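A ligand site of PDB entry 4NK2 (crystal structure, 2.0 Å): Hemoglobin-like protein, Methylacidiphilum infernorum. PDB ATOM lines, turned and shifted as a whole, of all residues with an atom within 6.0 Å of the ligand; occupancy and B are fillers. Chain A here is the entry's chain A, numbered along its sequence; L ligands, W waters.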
ATOM      1  N   ILE A  79      -2.810  10.063 -20.242  1.00  0.00           N
ATOM      2  CA  ILE A  79      -1.456  10.184 -19.689  1.00  0.00           C
ATOM      3  C   ILE A  79      -1.467  10.275 -18.167  1.00  0.00           C
ATOM      4  O   ILE A  79      -0.490  10.737 -17.556  1.00  0.00           O
ATOM      5  CB  ILE A  79      -0.671  11.382 -20.273  1.00  0.00           C
ATOM      6  CG1 ILE A  79      -1.437  12.697 -20.068  1.00  0.00           C
ATOM      7  CG2 ILE A  79      -0.343  11.143 -21.743  1.00  0.00           C
ATOM      8  CD1 ILE A  79      -0.632  13.956 -20.419  1.00  0.00           C
ATOM      9  N   LEU A  82       1.541   9.231 -15.944  1.00  0.00           N
ATOM     10  CA  LEU A  82       2.758  10.047 -15.816  1.00  0.00           C
ATOM     11  C   LEU A  82       2.806  10.860 -14.538  1.00  0.00           C
ATOM     12  O   LEU A  82       3.851  11.409 -14.182  1.00  0.00           O
ATOM     13  CB  LEU A  82       2.882  11.017 -16.993  1.00  0.00           C
ATOM     14  CG  LEU A  82       3.043  10.445 -18.392  1.00  0.00           C
ATOM     15  CD1 LEU A  82       3.194  11.582 -19.396  1.00  0.00           C
ATOM     16  CD2 LEU A  82       4.251   9.506 -18.441  1.00  0.00           C
ATOM     17  N   PHE A  83       1.661  10.944 -13.846  1.00  0.00           N
ATOM     18  CA  PHE A  83       1.521  11.880 -12.729  1.00  0.00           C
ATOM     19  C   PHE A  83       1.357  11.174 -11.403  1.00  0.00           C
ATOM     20  O   PHE A  83       0.984   9.995 -11.351  1.00  0.00           O
ATOM     21  CB  PHE A  83       0.337  12.816 -12.967  1.00  0.00           C
ATOM     22  CG  PHE A  83       0.481  13.629 -14.215  1.00  0.00           C
ATOM     23  CD1 PHE A  83       1.135  14.855 -14.190  1.00  0.00           C
ATOM     24  CD2 PHE A  83       0.011  13.139 -15.416  1.00  0.00           C
ATOM     25  CE1 PHE A  83       1.303  15.586 -15.343  1.00  0.00           C
ATOM     26  CE2 PHE A  83       0.166  13.877 -16.593  1.00  0.00           C
ATOM     27  CZ  PHE A  83       0.819  15.093 -16.554  1.00  0.00           C
ATOM     28  N   PRO A  84       1.635  11.886 -10.303  1.00  0.00           N
ATOM     29  CA  PRO A  84       1.632  11.212  -9.002  1.00  0.00           C
ATOM     30  C   PRO A  84       0.234  10.797  -8.572  1.00  0.00           C
ATOM     31  O   PRO A  84      -0.759  11.437  -8.916  1.00  0.00           O
ATOM     32  CB  PRO A  84       2.181  12.278  -8.044  1.00  0.00           C
ATOM     33  CG  PRO A  84       2.895  13.270  -8.925  1.00  0.00           C
ATOM     34  CD  PRO A  84       2.106  13.284 -10.202  1.00  0.00           C
ATOM     35  N   LEU A  93       3.251  19.174  -6.672  1.00  0.00           N
ATOM     36  CA  LEU A  93       3.384  19.506  -8.095  1.00  0.00           C
ATOM     37  C   LEU A  93       2.328  20.507  -8.571  1.00  0.00           C
ATOM     38  O   LEU A  93       2.644  21.410  -9.331  1.00  0.00           O
ATOM     39  CB  LEU A  93       3.358  18.236  -8.960  1.00  0.00           C
ATOM     40  CG  LEU A  93       4.523  17.258  -8.717  1.00  0.00           C
ATOM     41  CD1 LEU A  93       4.439  16.037  -9.611  1.00  0.00           C
ATOM     42  CD2 LEU A  93       5.866  17.956  -8.909  1.00  0.00           C
ATOM     43  N   ARG A  96       3.597  23.950  -7.490  1.00  0.00           N
ATOM     44  CA  ARG A  96       4.687  24.414  -8.339  1.00  0.00           C
ATOM     45  C   ARG A  96       4.174  24.923  -9.683  1.00  0.00           C
ATOM     46  O   ARG A  96       4.590  25.975 -10.147  1.00  0.00           O
ATOM     47  CB  ARG A  96       5.695  23.284  -8.604  1.00  0.00           C
ATOM     48  CG  ARG A  96       6.426  22.787  -7.362  1.00  0.00           C
ATOM     49  CD  ARG A  96       7.295  21.597  -7.688  1.00  0.00           C
ATOM     50  NE  ARG A  96       7.744  20.937  -6.469  1.00  0.00           N
ATOM     51  CZ  ARG A  96       8.546  19.886  -6.442  1.00  0.00           C
ATOM     52  NH1 ARG A  96       8.988  19.362  -7.574  1.00  0.00           N
ATOM     53  NH2 ARG A  96       8.906  19.358  -5.282  1.00  0.00           N
ATOM     54  N   SER A  97       3.286  24.159 -10.323  1.00  0.00           N
ATOM     55  CA  SER A  97       2.756  24.593 -11.607  1.00  0.00           C
ATOM     56  C   SER A  97       1.946  25.871 -11.473  1.00  0.00           C
ATOM     57  O   SER A  97       1.999  26.742 -12.347  1.00  0.00           O
ATOM     58  CB  SER A  97       1.861  23.515 -12.238  1.00  0.00           C
ATOM     59  OG  SER A  97       2.646  22.431 -12.677  1.00  0.00           O
ATOM     60  N   PHE A 100       4.231  28.733 -10.996  1.00  0.00           N
ATOM     61  CA  PHE A 100       4.844  29.071 -12.286  1.00  0.00           C
ATOM     62  C   PHE A 100       3.873  29.870 -13.178  1.00  0.00           C
ATOM     63  O   PHE A 100       4.239  30.893 -13.759  1.00  0.00           O
ATOM     64  CB  PHE A 100       5.289  27.790 -13.002  1.00  0.00           C
ATOM     65  CG  PHE A 100       5.992  28.031 -14.320  1.00  0.00           C
ATOM     66  CD1 PHE A 100       7.288  28.545 -14.348  1.00  0.00           C
ATOM     67  CD2 PHE A 100       5.359  27.746 -15.511  1.00  0.00           C
ATOM     68  CE1 PHE A 100       7.943  28.772 -15.555  1.00  0.00           C
ATOM     69  CE2 PHE A 100       5.996  27.992 -16.735  1.00  0.00           C
ATOM     70  CZ  PHE A 100       7.290  28.496 -16.748  1.00  0.00           C
ATOM     71  N   VAL A 101       2.642  29.381 -13.309  1.00  0.00           N
ATOM     72  CA  VAL A 101       1.654  30.048 -14.153  1.00  0.00           C
ATOM     73  C   VAL A 101       1.336  31.450 -13.664  1.00  0.00           C
ATOM     74  O   VAL A 101       1.267  32.391 -14.467  1.00  0.00           O
ATOM     75  CB  VAL A 101       0.341  29.233 -14.207  1.00  0.00           C
ATOM     76  CG1 VAL A 101      -0.791  30.090 -14.789  1.00  0.00           C
ATOM     77  CG2 VAL A 101       0.539  27.935 -15.031  1.00  0.00           C
ATOM     78  N   TYR A 111       7.346  31.335  -8.246  1.00  0.00           N
ATOM     79  CA  TYR A 111       8.115  30.166  -8.697  1.00  0.00           C
ATOM     80  C   TYR A 111       9.614  30.380  -8.563  1.00  0.00           C
ATOM     81  O   TYR A 111      10.335  29.525  -8.031  1.00  0.00           O
ATOM     82  CB  TYR A 111       7.750  29.782 -10.151  1.00  0.00           C
ATOM     83  CG  TYR A 111       8.429  28.508 -10.605  1.00  0.00           C
ATOM     84  CD1 TYR A 111       7.864  27.269 -10.348  1.00  0.00           C
ATOM     85  CD2 TYR A 111       9.650  28.537 -11.275  1.00  0.00           C
ATOM     86  CE1 TYR A 111       8.487  26.089 -10.751  1.00  0.00           C
ATOM     87  CE2 TYR A 111      10.281  27.363 -11.680  1.00  0.00           C
ATOM     88  CZ  TYR A 111       9.690  26.150 -11.401  1.00  0.00           C
ATOM     89  OH  TYR A 111      10.315  24.987 -11.799  1.00  0.00           O
ATOM     90  N   ARG A 115      11.234  27.349  -6.494  1.00  0.00           N
ATOM     91  CA  ARG A 115      11.917  26.333  -7.299  1.00  0.00           C
ATOM     92  C   ARG A 115      13.132  26.939  -8.010  1.00  0.00           C
ATOM     93  O   ARG A 115      14.116  26.230  -8.290  1.00  0.00           O
ATOM     94  CB  ARG A 115      10.949  25.705  -8.318  1.00  0.00           C
ATOM     95  CG  ARG A 115       9.751  24.968  -7.666  1.00  0.00           C
ATOM     96  CD  ARG A 115      10.193  23.720  -6.892  1.00  0.00           C
ATOM     97  NE  ARG A 115      10.780  22.714  -7.784  1.00  0.00           N
ATOM     98  CZ  ARG A 115      11.508  21.685  -7.370  1.00  0.00           C
ATOM     99  NH1 ARG A 115      11.751  21.501  -6.079  1.00  0.00           N
ATOM    100  NH2 ARG A 115      11.998  20.831  -8.253  1.00  0.00           N
ATOM    101  N   MET A 120      12.519  24.846 -18.070  1.00  0.00           N
ATOM    102  CA  MET A 120      11.429  23.909 -18.155  1.00  0.00           C
ATOM    103  C   MET A 120      11.717  22.665 -18.968  1.00  0.00           C
ATOM    104  O   MET A 120      11.345  21.590 -18.592  1.00  0.00           O
ATOM    105  CB  MET A 120      10.168  24.583 -18.680  1.00  0.00           C
ATOM    106  CG  MET A 120       9.294  25.224 -17.641  1.00  0.00           C
ATOM    107  SD  MET A 120       8.856  24.183 -16.265  1.00  0.00           S
ATOM    108  CE  MET A 120       9.306  25.230 -14.938  1.00  0.00           C
ATOM    109  N   ARG A 123      13.911  20.487 -16.780  1.00  0.00           N
ATOM    110  CA  ARG A 123      13.157  19.914 -15.659  1.00  0.00           C
ATOM    111  C   ARG A 123      12.251  18.782 -16.152  1.00  0.00           C
ATOM    112  O   ARG A 123      12.048  17.802 -15.419  1.00  0.00           O
ATOM    113  CB  ARG A 123      12.335  21.002 -14.933  1.00  0.00           C
ATOM    114  CG  ARG A 123      13.188  22.009 -14.137  1.00  0.00           C
ATOM    115  CD  ARG A 123      12.311  23.049 -13.415  1.00  0.00           C
ATOM    116  NE  ARG A 123      13.094  24.137 -12.797  1.00  0.00           N
ATOM    117  CZ  ARG A 123      13.488  24.157 -11.519  1.00  0.00           C
ATOM    118  NH1 ARG A 123      13.185  23.129 -10.724  1.00  0.00           N
ATOM    119  NH2 ARG A 123      14.176  25.182 -11.038  1.00  0.00           N
ATOM    120  N   HIS A 124      11.753  18.871 -17.374  1.00  0.00           N
ATOM    121  CA  HIS A 124      10.852  17.845 -17.886  1.00  0.00           C
ATOM    122  C   HIS A 124      11.542  16.579 -18.418  1.00  0.00           C
ATOM    123  O   HIS A 124      10.877  15.620 -18.732  1.00  0.00           O
ATOM    124  CB  HIS A 124       9.881  18.418 -18.919  1.00  0.00           C
ATOM    125  CG  HIS A 124       8.702  19.131 -18.320  1.00  0.00           C
ATOM    126  ND1 HIS A 124       8.774  20.436 -17.883  1.00  0.00           N
ATOM    127  CD2 HIS A 124       7.433  18.727 -18.087  1.00  0.00           C
ATOM    128  CE1 HIS A 124       7.603  20.801 -17.401  1.00  0.00           C
ATOM    129  NE2 HIS A 124       6.769  19.782 -17.521  1.00  0.00           N
ATOM    130  N   SER A 126      12.778  14.546 -16.712  1.00  0.00           N
ATOM    131  CA  SER A 126      12.422  13.556 -15.686  1.00  0.00           C
ATOM    132  C   SER A 126      11.143  12.768 -16.005  1.00  0.00           C
ATOM    133  O   SER A 126      10.711  11.932 -15.205  1.00  0.00           O
ATOM    134  CB  SER A 126      12.241  14.257 -14.333  1.00  0.00           C
ATOM    135  OG  SER A 126      13.406  14.991 -13.972  1.00  0.00           O
ATOM    136  N   VAL A 127      10.527  13.049 -17.136  1.00  0.00           N
ATOM    137  CA  VAL A 127       9.311  12.358 -17.523  1.00  0.00           C
ATOM    138  C   VAL A 127       9.284  12.187 -19.026  1.00  0.00           C
ATOM    139  O   VAL A 127       9.648  13.072 -19.758  1.00  0.00           O
ATOM    140  CB  VAL A 127       8.050  13.079 -17.011  1.00  0.00           C
ATOM    141  CG1 VAL A 127       8.070  14.515 -17.367  1.00  0.00           C
ATOM    142  CG2 VAL A 127       6.814  12.432 -17.531  1.00  0.00           C
ATOM    143  N   THR A 128       8.858  11.022 -19.490  1.00  0.00           N
ATOM    144  CA  THR A 128       8.909  10.740 -20.921  1.00  0.00           C
ATOM    145  C   THR A 128       7.716  11.405 -21.592  1.00  0.00           C
ATOM    146  O   THR A 128       6.570  11.102 -21.291  1.00  0.00           O
ATOM    147  CB  THR A 128       8.885   9.214 -21.181  1.00  0.00           C
ATOM    148  OG1 THR A 128       9.872   8.597 -20.345  1.00  0.00           O
ATOM    149  CG2 THR A 128       9.219   8.907 -22.626  1.00  0.00           C
ATOM    150  N   ILE A 129       7.990  12.328 -22.497  1.00  0.00           N
ATOM    151  CA  ILE A 129       6.905  13.092 -23.110  1.00  0.00           C
ATOM    152  C   ILE A 129       7.026  12.962 -24.619  1.00  0.00           C
ATOM    153  O   ILE A 129       7.966  13.499 -25.217  1.00  0.00           O
ATOM    154  CB  ILE A 129       6.980  14.593 -22.735  1.00  0.00           C
ATOM    155  CG1 ILE A 129       6.805  14.753 -21.205  1.00  0.00           C
ATOM    156  CG2 ILE A 129       5.884  15.397 -23.511  1.00  0.00           C
ATOM    157  CD1 ILE A 129       7.175  16.143 -20.663  1.00  0.00           C
ATOM    158  N   ALA A 133       1.445  12.753 -25.948  1.00  0.00           N
ATOM    159  CA  ALA A 133       1.366  13.286 -24.587  1.00  0.00           C
ATOM    160  C   ALA A 133       1.155  14.795 -24.575  1.00  0.00           C
ATOM    161  O   ALA A 133       0.347  15.318 -23.791  1.00  0.00           O
ATOM    162  CB  ALA A 133       2.627  12.943 -23.822  1.00  0.00           C
ATOM    163  N   ARG A 134       1.888  15.517 -25.420  1.00  0.00           N
ATOM    164  CA  ARG A 134       1.687  16.953 -25.520  1.00  0.00           C
ATOM    165  C   ARG A 134       0.288  17.290 -26.016  1.00  0.00           C
ATOM    166  O   ARG A 134      -0.352  18.221 -25.511  1.00  0.00           O
ATOM    167  CB  ARG A 134       2.722  17.621 -26.433  1.00  0.00           C
ATOM    168  CG  ARG A 134       2.234  18.970 -26.967  1.00  0.00           C
ATOM    169  CD  ARG A 134       3.295  19.703 -27.798  1.00  0.00           C
ATOM    170  NE  ARG A 134       2.775  20.952 -28.348  1.00  0.00           N
ATOM    171  CZ  ARG A 134       2.194  21.074 -29.549  1.00  0.00           C
ATOM    172  NH1 ARG A 134       2.068  20.017 -30.343  1.00  0.00           N
ATOM    173  NH2 ARG A 134       1.753  22.256 -29.947  1.00  0.00           N
ATOM    174  N   TRP A 137      -2.081  16.677 -23.110  1.00  0.00           N
ATOM    175  CA  TRP A 137      -1.869  17.730 -22.113  1.00  0.00           C
ATOM    176  C   TRP A 137      -2.552  19.025 -22.572  1.00  0.00           C
ATOM    177  O   TRP A 137      -3.199  19.712 -21.786  1.00  0.00           O
ATOM    178  CB  TRP A 137      -0.359  17.934 -21.923  1.00  0.00           C
ATOM    179  CG  TRP A 137       0.108  18.927 -20.863  1.00  0.00           C
ATOM    180  CD1 TRP A 137       0.519  18.650 -19.582  1.00  0.00           C
ATOM    181  CD2 TRP A 137       0.311  20.338 -21.041  1.00  0.00           C
ATOM    182  NE1 TRP A 137       0.931  19.795 -18.951  1.00  0.00           N
ATOM    183  CE2 TRP A 137       0.805  20.856 -19.819  1.00  0.00           C
ATOM    184  CE3 TRP A 137       0.095  21.223 -22.110  1.00  0.00           C
ATOM    185  CZ2 TRP A 137       1.097  22.201 -19.632  1.00  0.00           C
ATOM    186  CZ3 TRP A 137       0.387  22.567 -21.924  1.00  0.00           C
ATOM    187  CH2 TRP A 137       0.877  23.056 -20.701  1.00  0.00           C
ATOM    188  N   TRP A 161       0.714  30.852 -25.807  1.00  0.00           N
ATOM    189  CA  TRP A 161       1.881  30.581 -24.960  1.00  0.00           C
ATOM    190  C   TRP A 161       2.064  29.087 -24.712  1.00  0.00           C
ATOM    191  O   TRP A 161       3.115  28.522 -25.013  1.00  0.00           O
ATOM    192  CB  TRP A 161       1.791  31.326 -23.624  1.00  0.00           C
ATOM    193  CG  TRP A 161       2.883  30.927 -22.655  1.00  0.00           C
ATOM    194  CD1 TRP A 161       4.228  30.852 -22.926  1.00  0.00           C
ATOM    195  CD2 TRP A 161       2.734  30.565 -21.275  1.00  0.00           C
ATOM    196  NE1 TRP A 161       4.917  30.460 -21.786  1.00  0.00           N
ATOM    197  CE2 TRP A 161       4.009  30.279 -20.764  1.00  0.00           C
ATOM    198  CE3 TRP A 161       1.619  30.462 -20.419  1.00  0.00           C
ATOM    199  CZ2 TRP A 161       4.222  29.890 -19.441  1.00  0.00           C
ATOM    200  CZ3 TRP A 161       1.826  30.074 -19.117  1.00  0.00           C
ATOM    201  CH2 TRP A 161       3.131  29.791 -18.630  1.00  0.00           C
ATOM    202  N   ILE A 162       1.054  28.420 -24.161  1.00  0.00           N
ATOM    203  CA  ILE A 162       1.251  26.996 -23.864  1.00  0.00           C
ATOM    204  C   ILE A 162       1.315  26.111 -25.116  1.00  0.00           C
ATOM    205  O   ILE A 162       2.022  25.090 -25.120  1.00  0.00           O
ATOM    206  CB  ILE A 162       0.188  26.426 -22.880  1.00  0.00           C
ATOM    207  CG1 ILE A 162      -1.226  26.603 -23.445  1.00  0.00           C
ATOM    208  CG2 ILE A 162       0.304  27.105 -21.532  1.00  0.00           C
ATOM    209  CD1 ILE A 162      -2.308  25.869 -22.645  1.00  0.00           C
ATOM    210  N   PHE A 165       4.988  26.757 -26.201  1.00  0.00           N
ATOM    211  CA  PHE A 165       5.993  26.422 -25.191  1.00  0.00           C
ATOM    212  C   PHE A 165       6.012  24.919 -24.960  1.00  0.00           C
ATOM    213  O   PHE A 165       7.078  24.331 -24.721  1.00  0.00           O
ATOM    214  CB  PHE A 165       5.665  27.136 -23.874  1.00  0.00           C
ATOM    215  CG  PHE A 165       6.806  27.127 -22.879  1.00  0.00           C
ATOM    216  CD1 PHE A 165       8.128  27.114 -23.300  1.00  0.00           C
ATOM    217  CD2 PHE A 165       6.544  27.154 -21.512  1.00  0.00           C
ATOM    218  CE1 PHE A 165       9.167  27.130 -22.376  1.00  0.00           C
ATOM    219  CE2 PHE A 165       7.589  27.162 -20.586  1.00  0.00           C
ATOM    220  CZ  PHE A 165       8.897  27.147 -21.017  1.00  0.00           C
ATOM    221  N   SER A 166       4.849  24.286 -25.049  1.00  0.00           N
ATOM    222  CA  SER A 166       4.747  22.847 -24.808  1.00  0.00           C
ATOM    223  C   SER A 166       5.559  22.043 -25.819  1.00  0.00           C
ATOM    224  O   SER A 166       5.989  20.918 -25.537  1.00  0.00           O
ATOM    225  CB  SER A 166       3.273  22.386 -24.819  1.00  0.00           C
ATOM    226  OG  SER A 166       2.607  22.702 -26.038  1.00  0.00           O
ATOM    227  N   ILE A 167       5.795  22.601 -27.005  1.00  0.00           N
ATOM    228  CA  ILE A 167       6.583  21.843 -27.980  1.00  0.00           C
ATOM    229  C   ILE A 167       7.990  21.522 -27.457  1.00  0.00           C
ATOM    230  O   ILE A 167       8.552  20.464 -27.755  1.00  0.00           O
ATOM    231  CB  ILE A 167       6.696  22.598 -29.312  1.00  0.00           C
ATOM    232  CG1 ILE A 167       5.295  22.750 -29.943  1.00  0.00           C
ATOM    233  CG2 ILE A 167       7.598  21.852 -30.259  1.00  0.00           C
ATOM    234  CD1 ILE A 167       5.289  23.610 -31.195  1.00  0.00           C
ATOM    235  N   MET A 169       8.875  20.801 -24.526  1.00  0.00           N
ATOM    236  CA  MET A 169       8.928  19.787 -23.473  1.00  0.00           C
ATOM    237  C   MET A 169       9.070  18.376 -24.064  1.00  0.00           C
ATOM    238  O   MET A 169       9.412  17.427 -23.356  1.00  0.00           O
ATOM    239  CB  MET A 169       7.690  19.855 -22.604  1.00  0.00           C
ATOM    240  CG  MET A 169       7.408  21.267 -22.055  1.00  0.00           C
ATOM    241  SD  MET A 169       8.878  21.932 -21.245  1.00  0.00           S
ATOM    242  CE  MET A 169       8.590  23.625 -21.746  1.00  0.00           C
ATOM    243  N   ILE A 170       8.778  18.244 -25.366  1.00  0.00           N
ATOM    244  CA  ILE A 170       8.751  16.913 -25.985  1.00  0.00           C
ATOM    245  C   ILE A 170      10.169  16.340 -25.999  1.00  0.00           C
ATOM    246  O   ILE A 170      11.095  16.963 -26.554  1.00  0.00           O
ATOM    247  CB  ILE A 170       8.240  16.947 -27.443  1.00  0.00           C
ATOM    248  CG1 ILE A 170       6.757  17.362 -27.488  1.00  0.00           C
ATOM    249  CG2 ILE A 170       8.430  15.571 -28.090  1.00  0.00           C
ATOM    250  CD1 ILE A 170       6.218  17.538 -28.901  1.00  0.00           C
HETATM  251  C1  LIG L   1       6.216  19.278 -13.859  1.00  0.00           C
HETATM  252  C2  LIG L   1       4.033  16.712 -17.333  1.00  0.00           C
HETATM  253  C3  LIG L   1       4.306  20.565 -20.314  1.00  0.00           C
HETATM  254  C4  LIG L   1       4.754  23.257 -16.267  1.00  0.00           C
HETATM  255  C5  LIG L   1       5.694  18.208 -14.549  1.00  0.00           C
HETATM  256  C6  LIG L   1       5.698  16.813 -14.134  1.00  0.00           C
HETATM  257  C7  LIG L   1       5.076  16.114 -15.108  1.00  0.00           C
HETATM  258  C8  LIG L   1       4.679  17.042 -16.159  1.00  0.00           C
HETATM  259  C9  LIG L   1       4.797  14.598 -15.157  1.00  0.00           C
HETATM  260  C10 LIG L   1       6.305  16.257 -12.805  1.00  0.00           C
HETATM  261  C11 LIG L   1       7.726  15.751 -13.131  1.00  0.00           C
HETATM  262  C12 LIG L   1       8.538  15.201 -11.966  1.00  0.00           C
HETATM  263  O1  LIG L   1       9.171  14.120 -12.118  1.00  0.00           O
HETATM  264  O2  LIG L   1       8.578  15.822 -10.863  1.00  0.00           O
HETATM  265  C13 LIG L   1       3.984  17.477 -18.486  1.00  0.00           C
HETATM  266  C14 LIG L   1       3.651  17.024 -19.830  1.00  0.00           C
HETATM  267  C15 LIG L   1       3.730  18.083 -20.656  1.00  0.00           C
HETATM  268  C16 LIG L   1       4.112  19.256 -19.875  1.00  0.00           C
HETATM  269  C17 LIG L   1       3.244  15.595 -20.240  1.00  0.00           C
HETATM  270  C18 LIG L   1       3.441  18.039 -22.171  1.00  0.00           C
HETATM  271  C19 LIG L   1       3.834  19.054 -22.951  1.00  0.00           C
HETATM  272  C20 LIG L   1       4.399  21.667 -19.473  1.00  0.00           C
HETATM  273  C21 LIG L   1       4.352  23.070 -19.838  1.00  0.00           C
HETATM  274  C22 LIG L   1       4.489  23.808 -18.714  1.00  0.00           C
HETATM  275  C23 LIG L   1       4.615  22.893 -17.591  1.00  0.00           C
HETATM  276  C24 LIG L   1       4.204  23.622 -21.275  1.00  0.00           C
HETATM  277  C25 LIG L   1       4.483  25.346 -18.575  1.00  0.00           C
HETATM  278  C26 LIG L   1       3.961  26.138 -19.522  1.00  0.00           C
HETATM  279  C27 LIG L   1       5.313  22.485 -15.274  1.00  0.00           C
HETATM  280  C28 LIG L   1       5.924  22.967 -14.049  1.00  0.00           C
HETATM  281  C29 LIG L   1       6.360  21.716 -13.306  1.00  0.00           C
HETATM  282  C30 LIG L   1       5.994  20.600 -14.151  1.00  0.00           C
HETATM  283  C31 LIG L   1       6.090  24.426 -13.553  1.00  0.00           C
HETATM  284  C32 LIG L   1       7.100  21.662 -11.950  1.00  0.00           C
HETATM  285  C33 LIG L   1       8.584  21.877 -12.232  1.00  0.00           C
HETATM  286  C34 LIG L   1       9.312  21.827 -10.909  1.00  0.00           C
HETATM  287  O3  LIG L   1       9.441  20.715 -10.343  1.00  0.00           O
HETATM  288  O4  LIG L   1       9.762  22.899 -10.422  1.00  0.00           O
HETATM  289  N1  LIG L   1       5.069  18.311 -15.776  1.00  0.00           N
HETATM  290  N2  LIG L   1       4.257  18.831 -18.570  1.00  0.00           N
HETATM  291  N3  LIG L   1       4.555  21.617 -18.092  1.00  0.00           N
HETATM  292  N4  LIG L   1       5.375  21.106 -15.291  1.00  0.00           N
HETATM  293 FE1  LIG L   1       4.900  19.974 -16.981  1.00  0.00          FE
HETATM  294  O   HOH W   1       1.620  22.751 -15.716  1.00  0.00           O
HETATM  295  O   HOH W   2       9.646  18.115 -11.861  1.00  0.00           O
HETATM  296  O   HOH W   3       4.386  20.358 -11.281  1.00  0.00           O
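NE1 of Trp 137 sits close to N2 of the ligand.
O of Leu 82 touches C9 of the ligand (3.5 Å).
CE1 of Phe 83 touches C2 of the ligand, 3.6 Å away.
CD1 of Leu 93 touches C10 of the ligand, 3.7 Å away.
Ser 97 touches the ligand (OG to C28, 3.6 Å).
Phe 100 touches the ligand (CB to C31, 3.5 Å).
Met 120 touches the ligand (CE to C31, 3.6 Å).
CB of Ser 126 touches O1 of the ligand (3.8 Å).
CG2 of Val 127 touches C9 of the ligand, 3.8 Å away.
Ile 129 touches the ligand (CD1 to C14, 3.7 Å).
CB of Arg 134 touches C19 of the ligand (3.9 Å).
Trp 161 touches the ligand (CZ2 to C26, 3.8 Å).
Phe 165 touches the ligand (CD2 to C26, 3.4 Å).
CA of Ser 166 touches C24 of the ligand, 3.7 Å away.
Met 169 touches the ligand.
Within 4 Å of the ligand: Leu 82, Phe 83, Leu 93, Arg 96, Ser 97, Phe 100, Tyr 111, Arg 115, Met 120, Arg 123, His 124, Ser 126, Val 127, Ile 129, Arg 134, Trp 137, Trp 161, Phe 165, Ser 166 and Met 169.
Along chain A the residues within 4 Å of the ligand span positions 82 to 169.
The nearest printed residue that does not touch the ligand is Ile 79 (4.2 Å).
Water W3 lies within hydrogen-bond range of O of Leu 93 (2.8 Å) and OG of Ser 97 (3.0 Å).
FE1 of the ligand is bound by NE2 of His 124 (2.0 Å).
OH of Tyr 111 lies within hydrogen-bond range of O4 of the ligand.
The guanidinium group (NE) of Arg 115 is in salt-bridge range of an oxygen (O4) of the ligand (2.8 Å).
NH1 of Arg 96 lies within salt-bridge range of O3 of the ligand, 3.1 Å away.
The guanidinium group (NH1) of Arg 123 lies within salt-bridge range of an oxygen (O4) of the ligand.
A ring nitrogen (ND1) of His 124 sits at hydrogen-bond distance from the backbone carbonyl oxygen (O) of Met 120.
ND1 of His 124 sits at hydrogen-bond distance from SD of Met 169 (3.7 Å).
The side-chain hydroxyl (OH) of Tyr 111 sits at hydrogen-bond distance from the guanidinium group (NE) of Arg 123.
The backbone carbonyl oxygen (O) of Arg 115 lies within hydrogen-bond range of the guanidinium group (NH2) of Arg 123 (2.9 Å).
O of Arg 123 lies within hydrogen-bond range of OG of Ser 126, at 3.4 Å.
O of Leu 93 is in hydrogen-bond range of OG of Ser 97 (3.5 Å).
The guanidinium group (NE) of Arg 134 sits at hydrogen-bond distance from the side-chain hydroxyl (OG) of Ser 166 (2.9 Å).
OG of Ser 166 lies within hydrogen-bond range of O of Ile 162, at 2.6 Å.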
